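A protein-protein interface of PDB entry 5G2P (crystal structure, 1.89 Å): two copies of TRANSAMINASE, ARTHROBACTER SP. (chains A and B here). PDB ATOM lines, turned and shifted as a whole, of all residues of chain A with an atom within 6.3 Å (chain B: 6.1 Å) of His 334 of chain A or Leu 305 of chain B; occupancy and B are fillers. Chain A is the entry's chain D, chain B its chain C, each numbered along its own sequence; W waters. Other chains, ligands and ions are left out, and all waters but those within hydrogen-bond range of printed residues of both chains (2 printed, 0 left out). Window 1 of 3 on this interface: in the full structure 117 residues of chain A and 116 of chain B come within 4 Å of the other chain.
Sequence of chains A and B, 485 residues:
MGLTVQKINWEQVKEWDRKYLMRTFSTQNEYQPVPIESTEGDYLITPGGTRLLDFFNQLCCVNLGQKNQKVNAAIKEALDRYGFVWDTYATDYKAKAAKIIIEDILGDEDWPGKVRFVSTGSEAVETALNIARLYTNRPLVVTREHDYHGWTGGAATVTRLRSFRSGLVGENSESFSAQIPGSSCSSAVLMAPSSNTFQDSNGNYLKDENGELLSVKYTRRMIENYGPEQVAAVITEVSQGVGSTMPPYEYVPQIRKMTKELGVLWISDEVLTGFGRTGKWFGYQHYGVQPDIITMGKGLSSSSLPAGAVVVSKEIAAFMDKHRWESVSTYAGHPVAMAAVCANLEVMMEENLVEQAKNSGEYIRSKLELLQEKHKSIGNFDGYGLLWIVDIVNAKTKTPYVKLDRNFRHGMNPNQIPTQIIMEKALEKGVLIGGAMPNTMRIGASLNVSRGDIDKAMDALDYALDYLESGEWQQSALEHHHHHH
The backbone carbonyl oxygen (O) of Ser 304 of chain B sits at hydrogen-bond distance from a ring nitrogen (NE2) of His 334 of chain A.
O of Ser 303 of chain B sits at hydrogen-bond distance from NE2 of His 334 of chain A.
A ring nitrogen (ND1) of His 334 of chain A is in hydrogen-bond range of the backbone NH of Val 336 of chain A.
The backbone carbonyl oxygen of Ser 119 of chain B lies within hydrogen-bond range of the backbone NH of Ala 307 of chain B, at 3.0 Å.
O of Ser 301 of chain B sits at hydrogen-bond distance from OG of Ser 304 of chain B, at 2.7 Å.
O of Leu 305 of chain B sits at hydrogen-bond distance from OG of Ser 301 of chain B, 2.6 Å away.
The side-chain hydroxyl (OG) of Ser 301 of chain B sits close to the backbone NH (N) of Ser 303 of chain B, 3.4 Å away.
Among the printed residues, merely in contact across the chains: Leu 79 of chain A with Ile 75 of chain B, Phe 84 of chain A with Ser 303 of chain B, Leu 305 of chain A with Leu 305 of chain B, Tyr 331 of chain A with Ser 119 of chain B, Tyr 331 of chain A with Ser 301 of chain B, Tyr 331 of chain A with Ser 303 of chain B, Tyr 331 of chain A with Pro 306 of chain B, Tyr 331 of chain A with Ala 307 of chain B and His 334 of chain A with Leu 305 of chain B.
Of chain B, only Ser 303, Ser 304 and Leu 305 come within 4 Å of His 334 of chain A.
Of chain A, only Leu 305 and His 334 come within 4 Å of Leu 305 of chain B.
Printed residues of chain A within 4 Å of Ile 75 of chain B: Leu 79.
Of the printed residues of chain B, Phe 84 of chain A touches Ser 303.
Val 336 of chain B touches none of the printed residues of chain A.
Ala 339 of chain A touches none of the printed residues of chain B.
The nearest residue of chain A that does not touch Leu 305 of chain B is Val 336 of chain A (4.2 Å).
Printed residues of chain A that touch a printed residue of chain B: Leu 79, Phe 84, Leu 305, Tyr 331 and His 334.
Of the 13 printed residues of chain B, 8 touch a printed residue of chain A.
Hydrophobic or aromatic side chains of chain B that line the printed part of chain A: Ile 75, Leu 305 and Pro 306.
Among the printed residues, 11 pairs touch across the chains.
Among the printed residues, no Asp or Glu carboxylate lies within 4 Å of a Lys or Arg side-chain nitrogen of the other chain.
Leu 305 of chain A touches its own counterpart, Leu 305 of chain B.
Positions printed for both chains: 75, 119, 305, 306, 336 and 337.
Water W1 lies within hydrogen-bond range of OH of Tyr 331 of chain A, O of Ala 307 of chain B and OG of Ser 301 of chain B.
Water W2 lies within hydrogen-bond range of O of Ser 304 of chain B (2.8 Å) and O of Gly 83 of chain A (2.9 Å).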
ATOM      1  N   ILE A  75      23.595  12.420  32.537  1.00  0.00           N
ATOM      2  CA  ILE A  75      22.682  12.185  31.413  1.00  0.00           C
ATOM      3  C   ILE A  75      22.279  13.525  30.782  1.00  0.00           C
ATOM      4  O   ILE A  75      22.310  13.684  29.560  1.00  0.00           O
ATOM      5  CB  ILE A  75      21.430  11.369  31.821  1.00  0.00           C
ATOM      6  CG1 ILE A  75      21.839   9.962  32.298  1.00  0.00           C
ATOM      7  CG2 ILE A  75      20.445  11.301  30.657  1.00  0.00           C
ATOM      8  CD1 ILE A  75      20.763   9.224  33.076  1.00  0.00           C
ATOM      9  N   LEU A  79      23.011  14.944  26.817  1.00  0.00           N
ATOM     10  CA  LEU A  79      21.910  15.432  25.981  1.00  0.00           C
ATOM     11  C   LEU A  79      22.153  16.811  25.354  1.00  0.00           C
ATOM     12  O   LEU A  79      21.408  17.224  24.450  1.00  0.00           O
ATOM     13  CB  LEU A  79      20.593  15.414  26.778  1.00  0.00           C
ATOM     14  CG  LEU A  79      19.955  14.048  27.111  1.00  0.00           C
ATOM     15  CD1 LEU A  79      18.901  14.197  28.204  1.00  0.00           C
ATOM     16  CD2 LEU A  79      19.361  13.362  25.862  1.00  0.00           C
ATOM     17  N   TYR A  82      24.245  14.897  22.340  1.00  0.00           N
ATOM     18  CA  TYR A  82      23.551  13.804  21.643  1.00  0.00           C
ATOM     19  C   TYR A  82      22.039  13.832  21.923  1.00  0.00           C
ATOM     20  O   TYR A  82      21.625  14.298  22.988  1.00  0.00           O
ATOM     21  CB  TYR A  82      24.151  12.467  22.083  1.00  0.00           C
ATOM     22  CG  TYR A  82      25.634  12.318  21.782  1.00  0.00           C
ATOM     23  CD1 TYR A  82      26.090  12.111  20.477  1.00  0.00           C
ATOM     24  CD2 TYR A  82      26.576  12.360  22.807  1.00  0.00           C
ATOM     25  CE1 TYR A  82      27.445  11.961  20.202  1.00  0.00           C
ATOM     26  CE2 TYR A  82      27.936  12.207  22.553  1.00  0.00           C
ATOM     27  CZ  TYR A  82      28.366  12.001  21.249  1.00  0.00           C
ATOM     28  OH  TYR A  82      29.709  11.862  20.980  1.00  0.00           O
ATOM     29  N   GLY A  83      21.199  13.347  21.000  1.00  0.00           N
ATOM     30  CA  GLY A  83      21.601  12.777  19.719  1.00  0.00           C
ATOM     31  C   GLY A  83      21.701  11.254  19.748  1.00  0.00           C
ATOM     32  O   GLY A  83      21.541  10.629  20.809  1.00  0.00           O
ATOM     33  N   PHE A  84      21.987  10.665  18.586  1.00  0.00           N
ATOM     34  CA  PHE A  84      22.146   9.212  18.479  1.00  0.00           C
ATOM     35  C   PHE A  84      23.082   8.879  17.350  1.00  0.00           C
ATOM     36  O   PHE A  84      22.878   9.323  16.231  1.00  0.00           O
ATOM     37  CB  PHE A  84      20.816   8.508  18.197  1.00  0.00           C
ATOM     38  CG  PHE A  84      20.980   7.032  17.893  1.00  0.00           C
ATOM     39  CD1 PHE A  84      21.368   6.134  18.905  1.00  0.00           C
ATOM     40  CD2 PHE A  84      20.842   6.559  16.590  1.00  0.00           C
ATOM     41  CE1 PHE A  84      21.565   4.786  18.622  1.00  0.00           C
ATOM     42  CE2 PHE A  84      21.029   5.211  16.302  1.00  0.00           C
ATOM     43  CZ  PHE A  84      21.392   4.331  17.306  1.00  0.00           C
ATOM     44  N   VAL A  85      24.106   8.090  17.637  1.00  0.00           N
ATOM     45  CA  VAL A  85      24.830   7.413  16.550  1.00  0.00           C
ATOM     46  C   VAL A  85      24.809   5.920  16.875  1.00  0.00           C
ATOM     47  O   VAL A  85      24.772   5.538  18.063  1.00  0.00           O
ATOM     48  CB  VAL A  85      26.285   7.918  16.339  1.00  0.00           C
ATOM     49  CG1 VAL A  85      26.304   9.354  15.823  1.00  0.00           C
ATOM     50  CG2 VAL A  85      27.122   7.782  17.622  1.00  0.00           C
ATOM     51  N   THR A  91      32.245   7.136  20.119  1.00  0.00           N
ATOM     52  CA  THR A  91      31.984   8.261  21.032  1.00  0.00           C
ATOM     53  C   THR A  91      32.864   8.146  22.277  1.00  0.00           C
ATOM     54  O   THR A  91      33.331   7.050  22.622  1.00  0.00           O
ATOM     55  CB  THR A  91      30.511   8.361  21.535  1.00  0.00           C
ATOM     56  OG1 THR A  91      30.184   7.206  22.322  1.00  0.00           O
ATOM     57  CG2 THR A  91      29.504   8.505  20.376  1.00  0.00           C
ATOM     58  N   TYR A  93      31.767   8.554  25.432  1.00  0.00           N
ATOM     59  CA  TYR A  93      31.031   7.795  26.441  1.00  0.00           C
ATOM     60  C   TYR A  93      31.162   6.265  26.225  1.00  0.00           C
ATOM     61  O   TYR A  93      31.424   5.525  27.162  1.00  0.00           O
ATOM     62  CB  TYR A  93      29.564   8.203  26.458  1.00  0.00           C
ATOM     63  CG  TYR A  93      29.306   9.673  26.804  1.00  0.00           C
ATOM     64  CD1 TYR A  93      29.775  10.228  28.003  1.00  0.00           C
ATOM     65  CD2 TYR A  93      28.552  10.487  25.941  1.00  0.00           C
ATOM     66  CE1 TYR A  93      29.512  11.561  28.325  1.00  0.00           C
ATOM     67  CE2 TYR A  93      28.279  11.819  26.260  1.00  0.00           C
ATOM     68  CZ  TYR A  93      28.764  12.350  27.439  1.00  0.00           C
ATOM     69  OH  TYR A  93      28.493  13.666  27.747  1.00  0.00           O
ATOM     70  N   LYS A  94      31.011   5.810  24.987  1.00  0.00           N
ATOM     71  CA  LYS A  94      31.104   4.368  24.699  1.00  0.00           C
ATOM     72  C   LYS A  94      32.507   3.802  24.962  1.00  0.00           C
ATOM     73  O   LYS A  94      32.641   2.758  25.631  1.00  0.00           O
ATOM     74  CB  LYS A  94      30.628   4.073  23.277  1.00  0.00           C
ATOM     75  CG  LYS A  94      30.323   2.592  23.030  1.00  0.00           C
ATOM     76  CD  LYS A  94      29.819   2.397  21.615  1.00  0.00           C
ATOM     77  CE  LYS A  94      30.936   2.559  20.596  1.00  0.00           C
ATOM     78  NZ  LYS A  94      30.487   2.294  19.211  1.00  0.00           N
ATOM     79  N   PHE A 117      28.559  -3.477  23.896  1.00  0.00           N
ATOM     80  CA  PHE A 117      27.375  -2.945  24.589  1.00  0.00           C
ATOM     81  C   PHE A 117      26.119  -3.216  23.764  1.00  0.00           C
ATOM     82  O   PHE A 117      26.153  -3.108  22.535  1.00  0.00           O
ATOM     83  CB  PHE A 117      27.506  -1.436  24.869  1.00  0.00           C
ATOM     84  CG  PHE A 117      28.606  -1.094  25.861  1.00  0.00           C
ATOM     85  CD1 PHE A 117      28.427  -1.311  27.225  1.00  0.00           C
ATOM     86  CD2 PHE A 117      29.815  -0.546  25.422  1.00  0.00           C
ATOM     87  CE1 PHE A 117      29.430  -1.023  28.143  1.00  0.00           C
ATOM     88  CE2 PHE A 117      30.823  -0.235  26.340  1.00  0.00           C
ATOM     89  CZ  PHE A 117      30.633  -0.484  27.698  1.00  0.00           C
ATOM     90  N   SER A 119      21.425  -3.299  24.704  1.00  0.00           N
ATOM     91  CA  SER A 119      20.482  -2.520  25.503  1.00  0.00           C
ATOM     92  C   SER A 119      19.848  -3.214  26.694  1.00  0.00           C
ATOM     93  O   SER A 119      19.318  -2.531  27.556  1.00  0.00           O
ATOM     94  CB  SER A 119      19.359  -1.920  24.635  1.00  0.00           C
ATOM     95  OG  SER A 119      19.868  -1.054  23.632  1.00  0.00           O
ATOM     96  N   LEU A 305      19.365   4.072  32.595  1.00  0.00           N
ATOM     97  CA  LEU A 305      18.893   3.962  31.211  1.00  0.00           C
ATOM     98  C   LEU A 305      19.190   2.539  30.714  1.00  0.00           C
ATOM     99  O   LEU A 305      20.032   1.848  31.300  1.00  0.00           O
ATOM    100  CB  LEU A 305      19.587   4.989  30.311  1.00  0.00           C
ATOM    101  CG  LEU A 305      19.227   6.469  30.474  1.00  0.00           C
ATOM    102  CD1 LEU A 305      20.144   7.297  29.601  1.00  0.00           C
ATOM    103  CD2 LEU A 305      17.772   6.714  30.097  1.00  0.00           C
ATOM    104  N   PRO A 306      18.486   2.078  29.668  1.00  0.00           N
ATOM    105  CA  PRO A 306      18.679   0.671  29.286  1.00  0.00           C
ATOM    106  C   PRO A 306      20.091   0.405  28.752  1.00  0.00           C
ATOM    107  O   PRO A 306      20.537   1.083  27.836  1.00  0.00           O
ATOM    108  CB  PRO A 306      17.629   0.457  28.197  1.00  0.00           C
ATOM    109  CG  PRO A 306      16.538   1.431  28.554  1.00  0.00           C
ATOM    110  CD  PRO A 306      17.302   2.659  29.002  1.00  0.00           C
ATOM    111  N   THR A 330      20.360  -1.822  16.480  1.00  0.00           N
ATOM    112  CA  THR A 330      20.220  -0.366  16.269  1.00  0.00           C
ATOM    113  C   THR A 330      20.776   0.441  17.460  1.00  0.00           C
ATOM    114  O   THR A 330      21.643   1.308  17.272  1.00  0.00           O
ATOM    115  CB  THR A 330      18.760   0.056  15.971  1.00  0.00           C
ATOM    116  OG1 THR A 330      18.312  -0.634  14.810  1.00  0.00           O
ATOM    117  CG2 THR A 330      18.646   1.577  15.712  1.00  0.00           C
ATOM    118  N   TYR A 331      20.305   0.127  18.674  1.00  0.00           N
ATOM    119  CA  TYR A 331      20.609   0.944  19.853  1.00  0.00           C
ATOM    120  C   TYR A 331      21.849   0.495  20.638  1.00  0.00           C
ATOM    121  O   TYR A 331      22.172   1.082  21.683  1.00  0.00           O
ATOM    122  CB  TYR A 331      19.396   0.986  20.781  1.00  0.00           C
ATOM    123  CG  TYR A 331      18.209   1.659  20.145  1.00  0.00           C
ATOM    124  CD1 TYR A 331      18.383   2.767  19.325  1.00  0.00           C
ATOM    125  CD2 TYR A 331      16.908   1.224  20.397  1.00  0.00           C
ATOM    126  CE1 TYR A 331      17.296   3.406  18.750  1.00  0.00           C
ATOM    127  CE2 TYR A 331      15.812   1.887  19.842  1.00  0.00           C
ATOM    128  CZ  TYR A 331      16.025   2.977  19.022  1.00  0.00           C
ATOM    129  OH  TYR A 331      14.970   3.671  18.450  1.00  0.00           O
ATOM    130  N   ALA A 332      22.534  -0.541  20.145  1.00  0.00           N
ATOM    131  CA  ALA A 332      23.767  -1.015  20.775  1.00  0.00           C
ATOM    132  C   ALA A 332      24.752   0.157  20.835  1.00  0.00           C
ATOM    133  O   ALA A 332      25.054   0.765  19.802  1.00  0.00           O
ATOM    134  CB  ALA A 332      24.367  -2.176  19.971  1.00  0.00           C
ATOM    135  N   GLY A 333      25.206   0.488  22.043  1.00  0.00           N
ATOM    136  CA  GLY A 333      26.245   1.518  22.260  1.00  0.00           C
ATOM    137  C   GLY A 333      25.699   2.931  22.352  1.00  0.00           C
ATOM    138  O   GLY A 333      26.469   3.885  22.466  1.00  0.00           O
ATOM    139  N   HIS A 334      24.369   3.061  22.329  1.00  0.00           N
ATOM    140  CA  HIS A 334      23.667   4.352  22.414  1.00  0.00           C
ATOM    141  C   HIS A 334      24.422   5.338  23.314  1.00  0.00           C
ATOM    142  O   HIS A 334      24.574   5.072  24.505  1.00  0.00           O
ATOM    143  CB  HIS A 334      22.239   4.145  22.964  1.00  0.00           C
ATOM    144  CG  HIS A 334      21.354   5.332  22.767  1.00  0.00           C
ATOM    145  ND1 HIS A 334      21.560   6.530  23.421  1.00  0.00           N
ATOM    146  CD2 HIS A 334      20.283   5.524  21.958  1.00  0.00           C
ATOM    147  CE1 HIS A 334      20.655   7.406  23.023  1.00  0.00           C
ATOM    148  NE2 HIS A 334      19.868   6.820  22.137  1.00  0.00           N
ATOM    149  N   PRO A 335      24.876   6.482  22.754  1.00  0.00           N
ATOM    150  CA  PRO A 335      25.802   7.355  23.494  1.00  0.00           C
ATOM    151  C   PRO A 335      25.248   7.904  24.806  1.00  0.00           C
ATOM    152  O   PRO A 335      25.993   8.062  25.762  1.00  0.00           O
ATOM    153  CB  PRO A 335      26.086   8.488  22.505  1.00  0.00           C
ATOM    154  CG  PRO A 335      24.928   8.481  21.561  1.00  0.00           C
ATOM    155  CD  PRO A 335      24.592   7.016  21.410  1.00  0.00           C
ATOM    156  N   VAL A 336      23.944   8.141  24.876  1.00  0.00           N
ATOM    157  CA  VAL A 336      23.345   8.659  26.124  1.00  0.00           C
ATOM    158  C   VAL A 336      23.260   7.558  27.175  1.00  0.00           C
ATOM    159  O   VAL A 336      23.500   7.800  28.344  1.00  0.00           O
ATOM    160  CB  VAL A 336      21.974   9.332  25.901  1.00  0.00           C
ATOM    161  CG1 VAL A 336      21.452   9.894  27.218  1.00  0.00           C
ATOM    162  CG2 VAL A 336      22.083  10.447  24.857  1.00  0.00           C
ATOM    163  N   ALA A 337      22.934   6.333  26.755  1.00  0.00           N
ATOM    164  CA  ALA A 337      22.974   5.211  27.673  1.00  0.00           C
ATOM    165  C   ALA A 337      24.409   4.982  28.176  1.00  0.00           C
ATOM    166  O   ALA A 337      24.607   4.675  29.349  1.00  0.00           O
ATOM    167  CB  ALA A 337      22.405   3.940  27.022  1.00  0.00           C
ATOM    168  N   MET A 338      25.402   5.156  27.301  1.00  0.00           N
ATOM    169  CA  MET A 338      26.817   4.948  27.701  1.00  0.00           C
ATOM    170  C   MET A 338      27.240   6.035  28.706  1.00  0.00           C
ATOM    171  O   MET A 338      28.004   5.780  29.650  1.00  0.00           O
ATOM    172  CB  MET A 338      27.743   4.929  26.484  1.00  0.00           C
ATOM    173  CG  MET A 338      27.517   3.776  25.502  1.00  0.00           C
ATOM    174  SD  MET A 338      27.759   2.180  26.298  1.00  0.00           S
ATOM    175  CE  MET A 338      26.066   1.817  26.838  1.00  0.00           C
ATOM    176  N   ALA A 339      26.712   7.248  28.525  1.00  0.00           N
ATOM    177  CA  ALA A 339      26.992   8.318  29.491  1.00  0.00           C
ATOM    178  C   ALA A 339      26.489   7.960  30.869  1.00  0.00           C
ATOM    179  O   ALA A 339      27.172   8.198  31.882  1.00  0.00           O
ATOM    180  CB  ALA A 339      26.378   9.640  29.034  1.00  0.00           C
ATOM    181  N   ILE B  75      13.033  14.695  28.399  1.00  0.00           N
ATOM    182  CA  ILE B  75      13.847  13.694  29.088  1.00  0.00           C
ATOM    183  C   ILE B  75      14.400  14.260  30.396  1.00  0.00           C
ATOM    184  O   ILE B  75      14.351  13.591  31.435  1.00  0.00           O
ATOM    185  CB  ILE B  75      14.984  13.132  28.202  1.00  0.00           C
ATOM    186  CG1 ILE B  75      14.400  12.262  27.086  1.00  0.00           C
ATOM    187  CG2 ILE B  75      15.931  12.282  29.033  1.00  0.00           C
ATOM    188  CD1 ILE B  75      15.397  12.023  25.972  1.00  0.00           C
ATOM    189  N   SER B 119      12.542  -2.597  24.831  1.00  0.00           N
ATOM    190  CA  SER B 119      13.637  -1.634  24.633  1.00  0.00           C
ATOM    191  C   SER B 119      14.168  -1.518  23.213  1.00  0.00           C
ATOM    192  O   SER B 119      14.812  -0.515  22.886  1.00  0.00           O
ATOM    193  CB  SER B 119      14.793  -1.916  25.597  1.00  0.00           C
ATOM    194  OG  SER B 119      14.378  -1.701  26.954  1.00  0.00           O
ATOM    195  N   SER B 301      10.850   6.379  19.142  1.00  0.00           N
ATOM    196  CA  SER B 301      11.468   7.399  19.987  1.00  0.00           C
ATOM    197  C   SER B 301      12.434   8.270  19.187  1.00  0.00           C
ATOM    198  O   SER B 301      13.151   9.086  19.768  1.00  0.00           O
ATOM    199  CB  SER B 301      12.205   6.734  21.185  1.00  0.00           C
ATOM    200  OG  SER B 301      13.331   5.989  20.737  1.00  0.00           O
ATOM    201  N   SER B 302      12.459   8.087  17.859  1.00  0.00           N
ATOM    202  CA  SER B 302      13.516   8.629  16.968  1.00  0.00           C
ATOM    203  C   SER B 302      14.930   8.449  17.527  1.00  0.00           C
ATOM    204  O   SER B 302      15.777   9.361  17.416  1.00  0.00           O
ATOM    205  CB  SER B 302      13.270  10.106  16.639  1.00  0.00           C
ATOM    206  OG  SER B 302      12.059  10.253  15.929  1.00  0.00           O
ATOM    207  N   SER B 303      15.162   7.283  18.146  1.00  0.00           N
ATOM    208  CA  SER B 303      16.470   6.903  18.753  1.00  0.00           C
ATOM    209  C   SER B 303      16.927   7.761  19.918  1.00  0.00           C
ATOM    210  O   SER B 303      18.077   7.654  20.345  1.00  0.00           O
ATOM    211  CB  SER B 303      17.588   6.858  17.699  1.00  0.00           C
ATOM    212  OG  SER B 303      17.170   6.065  16.613  1.00  0.00           O
ATOM    213  N   SER B 304      16.045   8.602  20.448  1.00  0.00           N
ATOM    214  CA  SER B 304      16.454   9.511  21.513  1.00  0.00           C
ATOM    215  C   SER B 304      16.888   8.676  22.702  1.00  0.00           C
ATOM    216  O   SER B 304      17.923   8.941  23.295  1.00  0.00           O
ATOM    217  CB  SER B 304      15.341  10.499  21.885  1.00  0.00           C
ATOM    218  OG  SER B 304      14.121   9.847  22.207  1.00  0.00           O
ATOM    219  N   LEU B 305      16.088   7.654  23.022  1.00  0.00           N
ATOM    220  CA  LEU B 305      16.430   6.640  24.034  1.00  0.00           C
ATOM    221  C   LEU B 305      15.910   5.298  23.497  1.00  0.00           C
ATOM    222  O   LEU B 305      14.979   5.291  22.681  1.00  0.00           O
ATOM    223  CB  LEU B 305      15.792   6.988  25.406  1.00  0.00           C
ATOM    224  CG  LEU B 305      16.377   8.181  26.172  1.00  0.00           C
ATOM    225  CD1 LEU B 305      15.653   8.419  27.467  1.00  0.00           C
ATOM    226  CD2 LEU B 305      17.848   7.958  26.496  1.00  0.00           C
ATOM    227  N   PRO B 306      16.512   4.167  23.928  1.00  0.00           N
ATOM    228  CA  PRO B 306      16.036   2.852  23.439  1.00  0.00           C
ATOM    229  C   PRO B 306      14.576   2.572  23.808  1.00  0.00           C
ATOM    230  O   PRO B 306      14.198   2.626  24.998  1.00  0.00           O
ATOM    231  CB  PRO B 306      16.971   1.855  24.152  1.00  0.00           C
ATOM    232  CG  PRO B 306      18.216   2.650  24.439  1.00  0.00           C
ATOM    233  CD  PRO B 306      17.696   4.026  24.797  1.00  0.00           C
ATOM    234  N   ALA B 307      13.758   2.321  22.793  1.00  0.00           N
ATOM    235  CA  ALA B 307      12.380   1.861  22.987  1.00  0.00           C
ATOM    236  C   ALA B 307      11.969   0.984  21.806  1.00  0.00           C
ATOM    237  O   ALA B 307      12.375   1.227  20.667  1.00  0.00           O
ATOM    238  CB  ALA B 307      11.407   3.044  23.114  1.00  0.00           C
ATOM    239  N   VAL B 336      11.686   6.822  31.860  1.00  0.00           N
ATOM    240  CA  VAL B 336      12.417   7.889  31.180  1.00  0.00           C
ATOM    241  C   VAL B 336      12.392   7.650  29.651  1.00  0.00           C
ATOM    242  O   VAL B 336      12.254   8.597  28.866  1.00  0.00           O
ATOM    243  CB  VAL B 336      13.852   8.029  31.748  1.00  0.00           C
ATOM    244  CG1 VAL B 336      14.642   9.119  31.023  1.00  0.00           C
ATOM    245  CG2 VAL B 336      13.794   8.325  33.258  1.00  0.00           C
ATOM    246  N   ALA B 337      12.521   6.392  29.229  1.00  0.00           N
ATOM    247  CA  ALA B 337      12.384   6.067  27.801  1.00  0.00           C
ATOM    248  C   ALA B 337      10.972   6.428  27.329  1.00  0.00           C
ATOM    249  O   ALA B 337      10.793   6.914  26.219  1.00  0.00           O
ATOM    250  CB  ALA B 337      12.659   4.581  27.548  1.00  0.00           C
ATOM    251  N   ALA B 340      10.521  10.055  26.745  1.00  0.00           N
ATOM    252  CA  ALA B 340      11.131  10.368  25.461  1.00  0.00           C
ATOM    253  C   ALA B 340      10.187   9.978  24.345  1.00  0.00           C
ATOM    254  O   ALA B 340       9.999  10.760  23.412  1.00  0.00           O
ATOM    255  CB  ALA B 340      12.496   9.688  25.296  1.00  0.00           C
ATOM    256  N   VAL B 341       9.568   8.790  24.450  1.00  0.00           N
ATOM    257  CA  VAL B 341       8.558   8.389  23.455  1.00  0.00           C
ATOM    258  C   VAL B 341       7.404   9.393  23.385  1.00  0.00           C
ATOM    259  O   VAL B 341       7.041   9.840  22.296  1.00  0.00           O
ATOM    260  CB  VAL B 341       8.043   6.947  23.680  1.00  0.00           C
ATOM    261  CG1 VAL B 341       6.820   6.665  22.822  1.00  0.00           C
ATOM    262  CG2 VAL B 341       9.157   5.948  23.377  1.00  0.00           C
HETATM  263  O   HOH W   1      12.638   3.473  19.324  1.00  0.00           O
HETATM  264  O   HOH W   2      19.456  11.165  22.686  1.00  0.00           O
